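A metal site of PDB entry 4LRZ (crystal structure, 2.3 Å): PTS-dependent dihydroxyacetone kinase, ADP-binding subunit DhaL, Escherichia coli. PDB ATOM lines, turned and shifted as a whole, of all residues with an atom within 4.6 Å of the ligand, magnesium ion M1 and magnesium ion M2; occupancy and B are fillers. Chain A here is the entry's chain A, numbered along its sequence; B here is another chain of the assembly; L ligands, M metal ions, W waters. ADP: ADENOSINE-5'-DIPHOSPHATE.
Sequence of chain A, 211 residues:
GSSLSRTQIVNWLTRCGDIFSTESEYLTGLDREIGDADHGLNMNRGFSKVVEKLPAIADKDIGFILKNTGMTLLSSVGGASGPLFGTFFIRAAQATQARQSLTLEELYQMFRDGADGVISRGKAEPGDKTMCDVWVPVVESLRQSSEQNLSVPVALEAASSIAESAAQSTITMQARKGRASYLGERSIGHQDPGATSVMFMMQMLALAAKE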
ATOM      1  N   ASP A  31     -20.162 -17.044   5.485  1.00  0.00           N
ATOM      2  CA  ASP A  31     -18.778 -16.941   5.915  1.00  0.00           C
ATOM      3  C   ASP A  31     -18.693 -16.939   7.421  1.00  0.00           C
ATOM      4  O   ASP A  31     -17.617 -17.156   7.964  1.00  0.00           O
ATOM      5  CB  ASP A  31     -18.132 -15.640   5.362  1.00  0.00           C
ATOM      6  CG  ASP A  31     -16.555 -15.664   5.329  1.00  0.00           C
ATOM      7  OD1 ASP A  31     -15.955 -16.726   5.054  1.00  0.00           O
ATOM      8  OD2 ASP A  31     -15.895 -14.586   5.545  1.00  0.00           O
ATOM      9  N   ASP A  36     -14.327 -16.323   8.938  1.00  0.00           N
ATOM     10  CA  ASP A  36     -14.208 -15.160   9.829  1.00  0.00           C
ATOM     11  C   ASP A  36     -15.319 -14.130   9.631  1.00  0.00           C
ATOM     12  O   ASP A  36     -15.152 -12.956  10.007  1.00  0.00           O
ATOM     13  CB  ASP A  36     -12.827 -14.518   9.648  1.00  0.00           C
ATOM     14  CG  ASP A  36     -12.601 -14.013   8.226  1.00  0.00           C
ATOM     15  OD1 ASP A  36     -11.516 -13.459   7.927  1.00  0.00           O
ATOM     16  OD2 ASP A  36     -13.537 -14.163   7.401  1.00  0.00           O
ATOM     17  N   ALA A  37     -16.439 -14.528   9.039  1.00  0.00           N
ATOM     18  CA  ALA A  37     -17.619 -13.651   8.908  1.00  0.00           C
ATOM     19  C   ALA A  37     -17.372 -12.327   8.174  1.00  0.00           C
ATOM     20  O   ALA A  37     -17.803 -11.286   8.621  1.00  0.00           O
ATOM     21  CB  ALA A  37     -18.250 -13.347  10.357  1.00  0.00           C
ATOM     22  N   ASP A  38     -16.663 -12.340   7.055  1.00  0.00           N
ATOM     23  CA  ASP A  38     -16.355 -11.047   6.382  1.00  0.00           C
ATOM     24  C   ASP A  38     -16.579 -11.046   4.846  1.00  0.00           C
ATOM     25  O   ASP A  38     -16.540  -9.992   4.243  1.00  0.00           O
ATOM     26  CB  ASP A  38     -14.920 -10.622   6.709  1.00  0.00           C
ATOM     27  CG  ASP A  38     -13.901 -11.584   6.138  1.00  0.00           C
ATOM     28  OD1 ASP A  38     -14.281 -12.414   5.290  1.00  0.00           O
ATOM     29  OD2 ASP A  38     -12.700 -11.533   6.538  1.00  0.00           O
ATOM     30  N   HIS A  39     -16.812 -12.207   4.238  1.00  0.00           N
ATOM     31  CA  HIS A  39     -16.819 -12.297   2.767  1.00  0.00           C
ATOM     32  C   HIS A  39     -17.786 -11.374   2.060  1.00  0.00           C
ATOM     33  O   HIS A  39     -17.424 -10.699   1.104  1.00  0.00           O
ATOM     34  CB  HIS A  39     -17.029 -13.723   2.268  1.00  0.00           C
ATOM     35  CG  HIS A  39     -16.840 -13.872   0.780  1.00  0.00           C
ATOM     36  ND1 HIS A  39     -15.619 -13.700   0.162  1.00  0.00           N
ATOM     37  CD2 HIS A  39     -17.711 -14.203  -0.210  1.00  0.00           C
ATOM     38  CE1 HIS A  39     -15.749 -13.905  -1.137  1.00  0.00           C
ATOM     39  NE2 HIS A  39     -17.009 -14.223  -1.386  1.00  0.00           N
ATOM     40  N   ASN A  42     -16.430  -7.759   2.405  1.00  0.00           N
ATOM     41  CA  ASN A  42     -15.242  -7.508   1.595  1.00  0.00           C
ATOM     42  C   ASN A  42     -15.549  -7.481   0.089  1.00  0.00           C
ATOM     43  O   ASN A  42     -15.044  -6.641  -0.615  1.00  0.00           O
ATOM     44  CB  ASN A  42     -14.133  -8.508   1.937  1.00  0.00           C
ATOM     45  CG  ASN A  42     -13.625  -8.323   3.368  1.00  0.00           C
ATOM     46  OD1 ASN A  42     -12.817  -9.113   3.869  1.00  0.00           O
ATOM     47  ND2 ASN A  42     -14.113  -7.279   4.029  1.00  0.00           N
ATOM     48  N   GLY A  78      -9.075  -7.954   0.010  1.00  0.00           N
ATOM     49  CA  GLY A  78      -8.390  -8.531   1.146  1.00  0.00           C
ATOM     50  C   GLY A  78      -8.624 -10.033   1.264  1.00  0.00           C
ATOM     51  O   GLY A  78      -9.496 -10.595   0.578  1.00  0.00           O
ATOM     52  N   GLY A  79      -7.835 -10.657   2.124  1.00  0.00           N
ATOM     53  CA  GLY A  79      -7.936 -12.056   2.471  1.00  0.00           C
ATOM     54  C   GLY A  79      -7.617 -12.961   1.289  1.00  0.00           C
ATOM     55  O   GLY A  79      -6.924 -12.569   0.347  1.00  0.00           O
ATOM     56  N   ALA A  80      -8.150 -14.179   1.351  1.00  0.00           N
ATOM     57  CA  ALA A  80      -7.907 -15.190   0.321  1.00  0.00           C
ATOM     58  C   ALA A  80      -8.606 -14.817  -0.960  1.00  0.00           C
ATOM     59  O   ALA A  80      -8.044 -15.019  -1.997  1.00  0.00           O
ATOM     60  CB  ALA A  80      -8.337 -16.550   0.798  1.00  0.00           C
ATOM     61  N   SER A  81      -9.790 -14.211  -0.923  1.00  0.00           N
ATOM     62  CA  SER A  81     -10.562 -14.092  -2.178  1.00  0.00           C
ATOM     63  C   SER A  81     -10.148 -12.927  -3.049  1.00  0.00           C
ATOM     64  O   SER A  81     -10.265 -12.997  -4.276  1.00  0.00           O
ATOM     65  CB  SER A  81     -12.074 -14.086  -1.936  1.00  0.00           C
ATOM     66  OG  SER A  81     -12.415 -12.991  -1.136  1.00  0.00           O
ATOM     67  N   LEU A  84      -7.460 -13.783  -5.524  1.00  0.00           N
ATOM     68  CA  LEU A  84      -8.014 -14.724  -6.440  1.00  0.00           C
ATOM     69  C   LEU A  84      -8.994 -14.078  -7.465  1.00  0.00           C
ATOM     70  O   LEU A  84      -8.882 -14.269  -8.696  1.00  0.00           O
ATOM     71  CB  LEU A  84      -8.615 -15.899  -5.659  1.00  0.00           C
ATOM     72  CG  LEU A  84      -7.589 -16.649  -4.753  1.00  0.00           C
ATOM     73  CD1 LEU A  84      -8.287 -17.687  -3.948  1.00  0.00           C
ATOM     74  CD2 LEU A  84      -6.432 -17.330  -5.510  1.00  0.00           C
ATOM     75  N   GLY A 122      -3.942 -20.213  -6.396  1.00  0.00           N
ATOM     76  CA  GLY A 122      -4.446 -20.770  -5.147  1.00  0.00           C
ATOM     77  C   GLY A 122      -4.306 -22.293  -4.931  1.00  0.00           C
ATOM     78  O   GLY A 122      -4.533 -22.801  -3.819  1.00  0.00           O
ATOM     79  N   ALA A 124      -5.974 -24.848  -5.757  1.00  0.00           N
ATOM     80  CA  ALA A 124      -7.154 -25.590  -5.323  1.00  0.00           C
ATOM     81  C   ALA A 124      -7.466 -26.719  -6.318  1.00  0.00           C
ATOM     82  O   ALA A 124      -7.182 -26.603  -7.513  1.00  0.00           O
ATOM     83  CB  ALA A 124      -8.342 -24.653  -5.152  1.00  0.00           C
ATOM     84  N   THR A 130     -13.934 -24.741  -2.608  1.00  0.00           N
ATOM     85  CA  THR A 130     -13.537 -23.349  -2.854  1.00  0.00           C
ATOM     86  C   THR A 130     -14.287 -22.846  -4.059  1.00  0.00           C
ATOM     87  O   THR A 130     -15.097 -23.554  -4.620  1.00  0.00           O
ATOM     88  CB  THR A 130     -12.022 -23.185  -3.138  1.00  0.00           C
ATOM     89  OG1 THR A 130     -11.737 -23.660  -4.471  1.00  0.00           O
ATOM     90  CG2 THR A 130     -11.133 -23.896  -2.095  1.00  0.00           C
ATOM     91  N   MET A 131     -13.961 -21.625  -4.478  1.00  0.00           N
ATOM     92  CA  MET A 131     -14.521 -20.986  -5.664  1.00  0.00           C
ATOM     93  C   MET A 131     -14.163 -21.732  -6.958  1.00  0.00           C
ATOM     94  O   MET A 131     -14.824 -21.551  -8.005  1.00  0.00           O
ATOM     95  CB  MET A 131     -14.064 -19.537  -5.747  1.00  0.00           C
ATOM     96  CG  MET A 131     -12.528 -19.370  -5.837  1.00  0.00           C
ATOM     97  SD  MET A 131     -11.989 -17.706  -6.351  1.00  0.00           S
ATOM     98  CE  MET A 131     -12.287 -16.710  -4.872  1.00  0.00           C
ATOM     99  N   CYS A 132     -13.100 -22.544  -6.915  1.00  0.00           N
ATOM    100  CA  CYS A 132     -12.687 -23.283  -8.132  1.00  0.00           C
ATOM    101  C   CYS A 132     -13.648 -24.434  -8.413  1.00  0.00           C
ATOM    102  O   CYS A 132     -13.734 -24.931  -9.553  1.00  0.00           O
ATOM    103  CB  CYS A 132     -11.254 -23.800  -8.017  1.00  0.00           C
ATOM    104  SG  CYS A 132     -10.081 -22.456  -7.921  1.00  0.00           S
ATOM    105  N   LYS A 177      -8.871 -26.173   1.652  1.00  0.00           N
ATOM    106  CA  LYS A 177      -8.145 -24.905   1.485  1.00  0.00           C
ATOM    107  C   LYS A 177      -8.816 -23.781   2.245  1.00  0.00           C
ATOM    108  O   LYS A 177     -10.018 -23.840   2.528  1.00  0.00           O
ATOM    109  CB  LYS A 177      -7.995 -24.473   0.019  1.00  0.00           C
ATOM    110  CG  LYS A 177      -7.247 -25.466  -0.895  1.00  0.00           C
ATOM    111  CD  LYS A 177      -5.741 -25.310  -0.849  1.00  0.00           C
ATOM    112  CE  LYS A 177      -5.082 -26.138  -1.940  1.00  0.00           C
ATOM    113  NZ  LYS A 177      -5.306 -27.584  -1.714  1.00  0.00           N
ATOM    114  N   GLY A 178      -8.026 -22.771   2.578  1.00  0.00           N
ATOM    115  CA  GLY A 178      -8.555 -21.555   3.152  1.00  0.00           C
ATOM    116  C   GLY A 178      -9.040 -21.766   4.568  1.00  0.00           C
ATOM    117  O   GLY A 178      -8.848 -22.797   5.179  1.00  0.00           O
ATOM    118  N   ARG A 179      -9.692 -20.746   5.072  1.00  0.00           N
ATOM    119  CA  ARG A 179     -10.075 -20.649   6.454  1.00  0.00           C
ATOM    120  C   ARG A 179     -11.009 -21.758   6.934  1.00  0.00           C
ATOM    121  O   ARG A 179     -10.947 -22.190   8.083  1.00  0.00           O
ATOM    122  CB  ARG A 179     -10.760 -19.307   6.631  1.00  0.00           C
ATOM    123  CG  ARG A 179      -9.810 -18.123   6.641  1.00  0.00           C
ATOM    124  CD  ARG A 179      -9.666 -17.817   8.055  1.00  0.00           C
ATOM    125  NE  ARG A 179      -9.683 -16.416   8.323  1.00  0.00           N
ATOM    126  CZ  ARG A 179      -9.281 -15.908   9.478  1.00  0.00           C
ATOM    127  NH1 ARG A 179      -8.884 -16.729  10.443  1.00  0.00           N
ATOM    128  NH2 ARG A 179      -9.268 -14.592   9.650  1.00  0.00           N
ATOM    129  N   ASP A 192     -20.051 -22.956   0.552  1.00  0.00           N
ATOM    130  CA  ASP A 192     -18.856 -22.089   0.441  1.00  0.00           C
ATOM    131  C   ASP A 192     -19.207 -20.684  -0.069  1.00  0.00           C
ATOM    132  O   ASP A 192     -19.839 -20.553  -1.099  1.00  0.00           O
ATOM    133  CB  ASP A 192     -17.832 -22.698  -0.497  1.00  0.00           C
ATOM    134  CG  ASP A 192     -16.510 -21.928  -0.513  1.00  0.00           C
ATOM    135  OD1 ASP A 192     -15.830 -21.932   0.567  1.00  0.00           O
ATOM    136  OD2 ASP A 192     -16.168 -21.291  -1.568  1.00  0.00           O
ATOM    137  N   PRO A 193     -18.801 -19.631   0.641  1.00  0.00           N
ATOM    138  CA  PRO A 193     -19.084 -18.235   0.177  1.00  0.00           C
ATOM    139  C   PRO A 193     -18.339 -17.804  -1.094  1.00  0.00           C
ATOM    140  O   PRO A 193     -18.903 -17.094  -1.930  1.00  0.00           O
ATOM    141  CB  PRO A 193     -18.683 -17.323   1.362  1.00  0.00           C
ATOM    142  CG  PRO A 193     -17.963 -18.205   2.367  1.00  0.00           C
ATOM    143  CD  PRO A 193     -18.198 -19.692   1.993  1.00  0.00           C
ATOM    144  N   GLY A 194     -17.083 -18.183  -1.256  1.00  0.00           N
ATOM    145  CA  GLY A 194     -16.437 -17.821  -2.518  1.00  0.00           C
ATOM    146  C   GLY A 194     -17.186 -18.412  -3.721  1.00  0.00           C
ATOM    147  O   GLY A 194     -17.358 -17.706  -4.755  1.00  0.00           O
ATOM    148  N   ALA A 195     -17.661 -19.673  -3.591  1.00  0.00           N
ATOM    149  CA  ALA A 195     -18.378 -20.351  -4.671  1.00  0.00           C
ATOM    150  C   ALA A 195     -19.738 -19.672  -4.960  1.00  0.00           C
ATOM    151  O   ALA A 195     -20.146 -19.567  -6.121  1.00  0.00           O
ATOM    152  CB  ALA A 195     -18.582 -21.839  -4.379  1.00  0.00           C
ATOM    153  N   GLU B  66      -4.632 -11.033  10.492  1.00  0.00           N
ATOM    154  CA  GLU B  66      -4.805 -12.456  10.195  1.00  0.00           C
ATOM    155  C   GLU B  66      -3.529 -13.292  10.397  1.00  0.00           C
ATOM    156  O   GLU B  66      -3.600 -14.319  11.030  1.00  0.00           O
ATOM    157  CB  GLU B  66      -5.319 -12.649   8.763  1.00  0.00           C
ATOM    158  CG  GLU B  66      -5.682 -14.129   8.479  1.00  0.00           C
ATOM    159  CD  GLU B  66      -5.836 -14.472   6.986  1.00  0.00           C
ATOM    160  OE1 GLU B  66      -5.862 -15.697   6.678  1.00  0.00           O
ATOM    161  OE2 GLU B  66      -5.949 -13.531   6.154  1.00  0.00           O
HETATM  162  PB  ADP L   1     -10.937 -14.942   4.050  1.00  0.00           P
HETATM  163  O1B ADP L   1     -11.578 -14.093   5.101  1.00  0.00           O
HETATM  164  O2B ADP L   1      -9.470 -14.636   3.989  1.00  0.00           O
HETATM  165  O3B ADP L   1     -11.283 -16.387   4.152  1.00  0.00           O
HETATM  166  PA  ADP L   1     -12.956 -14.415   2.161  1.00  0.00           P
HETATM  167  O1A ADP L   1     -13.844 -14.616   3.349  1.00  0.00           O
HETATM  168  O2A ADP L   1     -13.150 -13.199   1.293  1.00  0.00           O
HETATM  169  O3A ADP L   1     -11.435 -14.394   2.635  1.00  0.00           O
HETATM  170  O5' ADP L   1     -12.987 -15.657   1.183  1.00  0.00           O
HETATM  171  C5' ADP L   1     -13.265 -17.011   1.548  1.00  0.00           C
HETATM  172  C4' ADP L   1     -13.364 -17.810   0.256  1.00  0.00           C
HETATM  173  O4' ADP L   1     -12.095 -17.814  -0.389  1.00  0.00           O
HETATM  174  C3' ADP L   1     -13.681 -19.284   0.505  1.00  0.00           C
HETATM  175  O3' ADP L   1     -15.113 -19.459   0.533  1.00  0.00           O
HETATM  176  C2' ADP L   1     -13.047 -19.949  -0.680  1.00  0.00           C
HETATM  177  O2' ADP L   1     -14.024 -19.980  -1.735  1.00  0.00           O
HETATM  178  C1' ADP L   1     -11.948 -19.002  -1.167  1.00  0.00           C
HETATM  179  N9  ADP L   1     -10.583 -19.578  -1.071  1.00  0.00           N
HETATM  180  C8  ADP L   1      -9.797 -19.671   0.025  1.00  0.00           C
HETATM  181  N7  ADP L   1      -8.606 -20.266  -0.297  1.00  0.00           N
HETATM  182  C5  ADP L   1      -8.658 -20.586  -1.606  1.00  0.00           C
HETATM  183  C6  ADP L   1      -7.751 -21.216  -2.579  1.00  0.00           C
HETATM  184  N6  ADP L   1      -6.546 -21.689  -2.237  1.00  0.00           N
HETATM  185  N1  ADP L   1      -8.196 -21.339  -3.824  1.00  0.00           N
HETATM  186  C2  ADP L   1      -9.409 -20.898  -4.222  1.00  0.00           C
HETATM  187  N3  ADP L   1     -10.275 -20.302  -3.383  1.00  0.00           N
HETATM  188  C4  ADP L   1      -9.955 -20.127  -2.097  1.00  0.00           C
HETATM  189 MG    MG M   1     -13.743 -14.538   5.344  1.00  0.00          MG
HETATM  190 MG    MG M   2     -10.788 -12.236   6.283  1.00  0.00          MG
HETATM  191  O   HOH W   1     -10.722 -11.290   4.668  1.00  0.00           O
HETATM  192  O   HOH W   2     -11.793 -10.924   2.282  1.00  0.00           O
HETATM  193  O   HOH W   3      -9.175 -13.431   6.213  1.00  0.00           O
HETATM  194  O   HOH W   4      -6.531 -19.600   1.196  1.00  0.00           O
HETATM  195  O   HOH W   5     -14.990 -19.638   3.901  1.00  0.00           O
HETATM  196  O   HOH W   6      -7.030 -22.097  -6.216  1.00  0.00           O
HETATM  197  O   HOH W   7     -13.358 -16.456   5.452  1.00  0.00           O
HETATM  198  O   HOH W   8     -10.225 -18.668   3.208  1.00  0.00           O
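ND1 of His 39 lies within hydrogen-bond range of O2A of the ligand (2.8 Å). A nitrogen (N6) of the ligand sits at hydrogen-bond distance from the backbone carbonyl oxygen (O) of Gly 122 (2.8 Å). OD2 of Asp 192 sits at hydrogen-bond distance from O2' of the ligand, at 2.5 Å. N of Gly 194 is in hydrogen-bond range of O3' of the ligand, at 3.0 Å. O2A of the ligand sits at hydrogen-bond distance from OG of Ser 81, 2.5 Å away. The backbone NH (N) of Met 131 sits at hydrogen-bond distance from an oxygen (O2') of the ligand (3.2 Å). The backbone NH (N) of Ala 80 is in hydrogen-bond range of an oxygen (O2B) of the ligand.
The backbone carbonyl oxygen (O) of Asp 31 sits at hydrogen-bond distance from the backbone NH (N) of Ala 37, 3.1 Å away. The backbone NH of Ala 195 sits at hydrogen-bond distance from the side-chain carboxylate of Asp 192, at 3.0 Å. N of Cys 132 is in hydrogen-bond range of OG1 of Thr 130 (3.0 Å). The backbone NH (N) of Gly 194 is in hydrogen-bond range of the side-chain carboxylate (OD2) of Asp 192, 3.3 Å away. NH2 of Arg 179 sits close to OD1 of Asp 36, at 3.1 Å. OD2 of Asp 31 lies close to N of His 39 (2.9 Å). NE2 of His 39 lies within hydrogen-bond range of O of Pro 193, 3.5 Å away.
Residues that only touch the ligand: Leu 84, Gly 79, Arg 179, Thr 130, Pro 193, Ala 124, Gly 178 and Lys 177. Hydrophobic or aromatic side chains that line the ligand: His 39, Ala 80, Leu 84, Ala 124, Met 131 and Pro 193. 18 residues have an atom within 4 Å of the ligand: Asp 31, Asp 36, Asp 38, His 39, Gly 79, Ala 80, Ser 81, Leu 84, Gly 122, Ala 124, Thr 130, Met 131, Lys 177, Gly 178, Arg 179, Asp 192, Pro 193 and Gly 194.
Of the 24 residues printed, 3 come within 4 Å of magnesium ion M1. Along chain A the residues within 4 Å of magnesium ion M1 span positions 31 to 38. The nearest printed residue that does not touch magnesium ion M1 is His 39 (4.01 Å).
Of the 24 residues printed, 2 come within 4 Å of magnesium ion M2.
Magnesium ion M1 is bound by water W7 (2.0 Å), an oxygen (O1A) of the ligand (2.0 Å), the side-chain carboxylate of Asp 36 (2.1 Å), the side-chain carboxylate of Asp 31 (2.2 Å), the side-chain carboxylate of Asp 38 (2.2 Å) and an oxygen (O1B) of the ligand (2.2 Å). Magnesium ion M1 has six donor atoms within binding distance.
Water W1 binds magnesium ion M2, at 1.9 Å. Water W3 binds magnesium ion M2 (2.0 Å). OD2 of Asp 38 binds magnesium ion M2. OD1 of Asp 36 binds magnesium ion M2, 2.2 Å away. Magnesium ion M2 is bound by O1B of the ligand.
Water W7 lies within hydrogen-bond range of an oxygen (O3B) of the ligand (2.4 Å) and the side-chain carboxylate (OD1) of Asp 31 (2.6 Å). Water W3 bridges O2B of the ligand (2.5 Å) and OE2 of Glu 66 of chain B (3.2 Å). Water W8 bridges O3B of the ligand (2.7 Å) and N of Arg 179 (2.8 Å). Water W6 lies within hydrogen-bond range of a nitrogen (N1) of the ligand (2.8 Å), the backbone NH (N) of Ala 124 (3.0 Å) and the side-chain sulfur (SG) of Cys 132 (3.5 Å). Water W2 lies within hydrogen-bond range of OD1 of Asn 42 (2.6 Å), O2A of the ligand (2.8 Å) and O of Gly 78 (2.9 Å). Water W5 bridges OD1 of Asp 31 (3.3 Å) and O3' of the ligand (3.4 Å).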
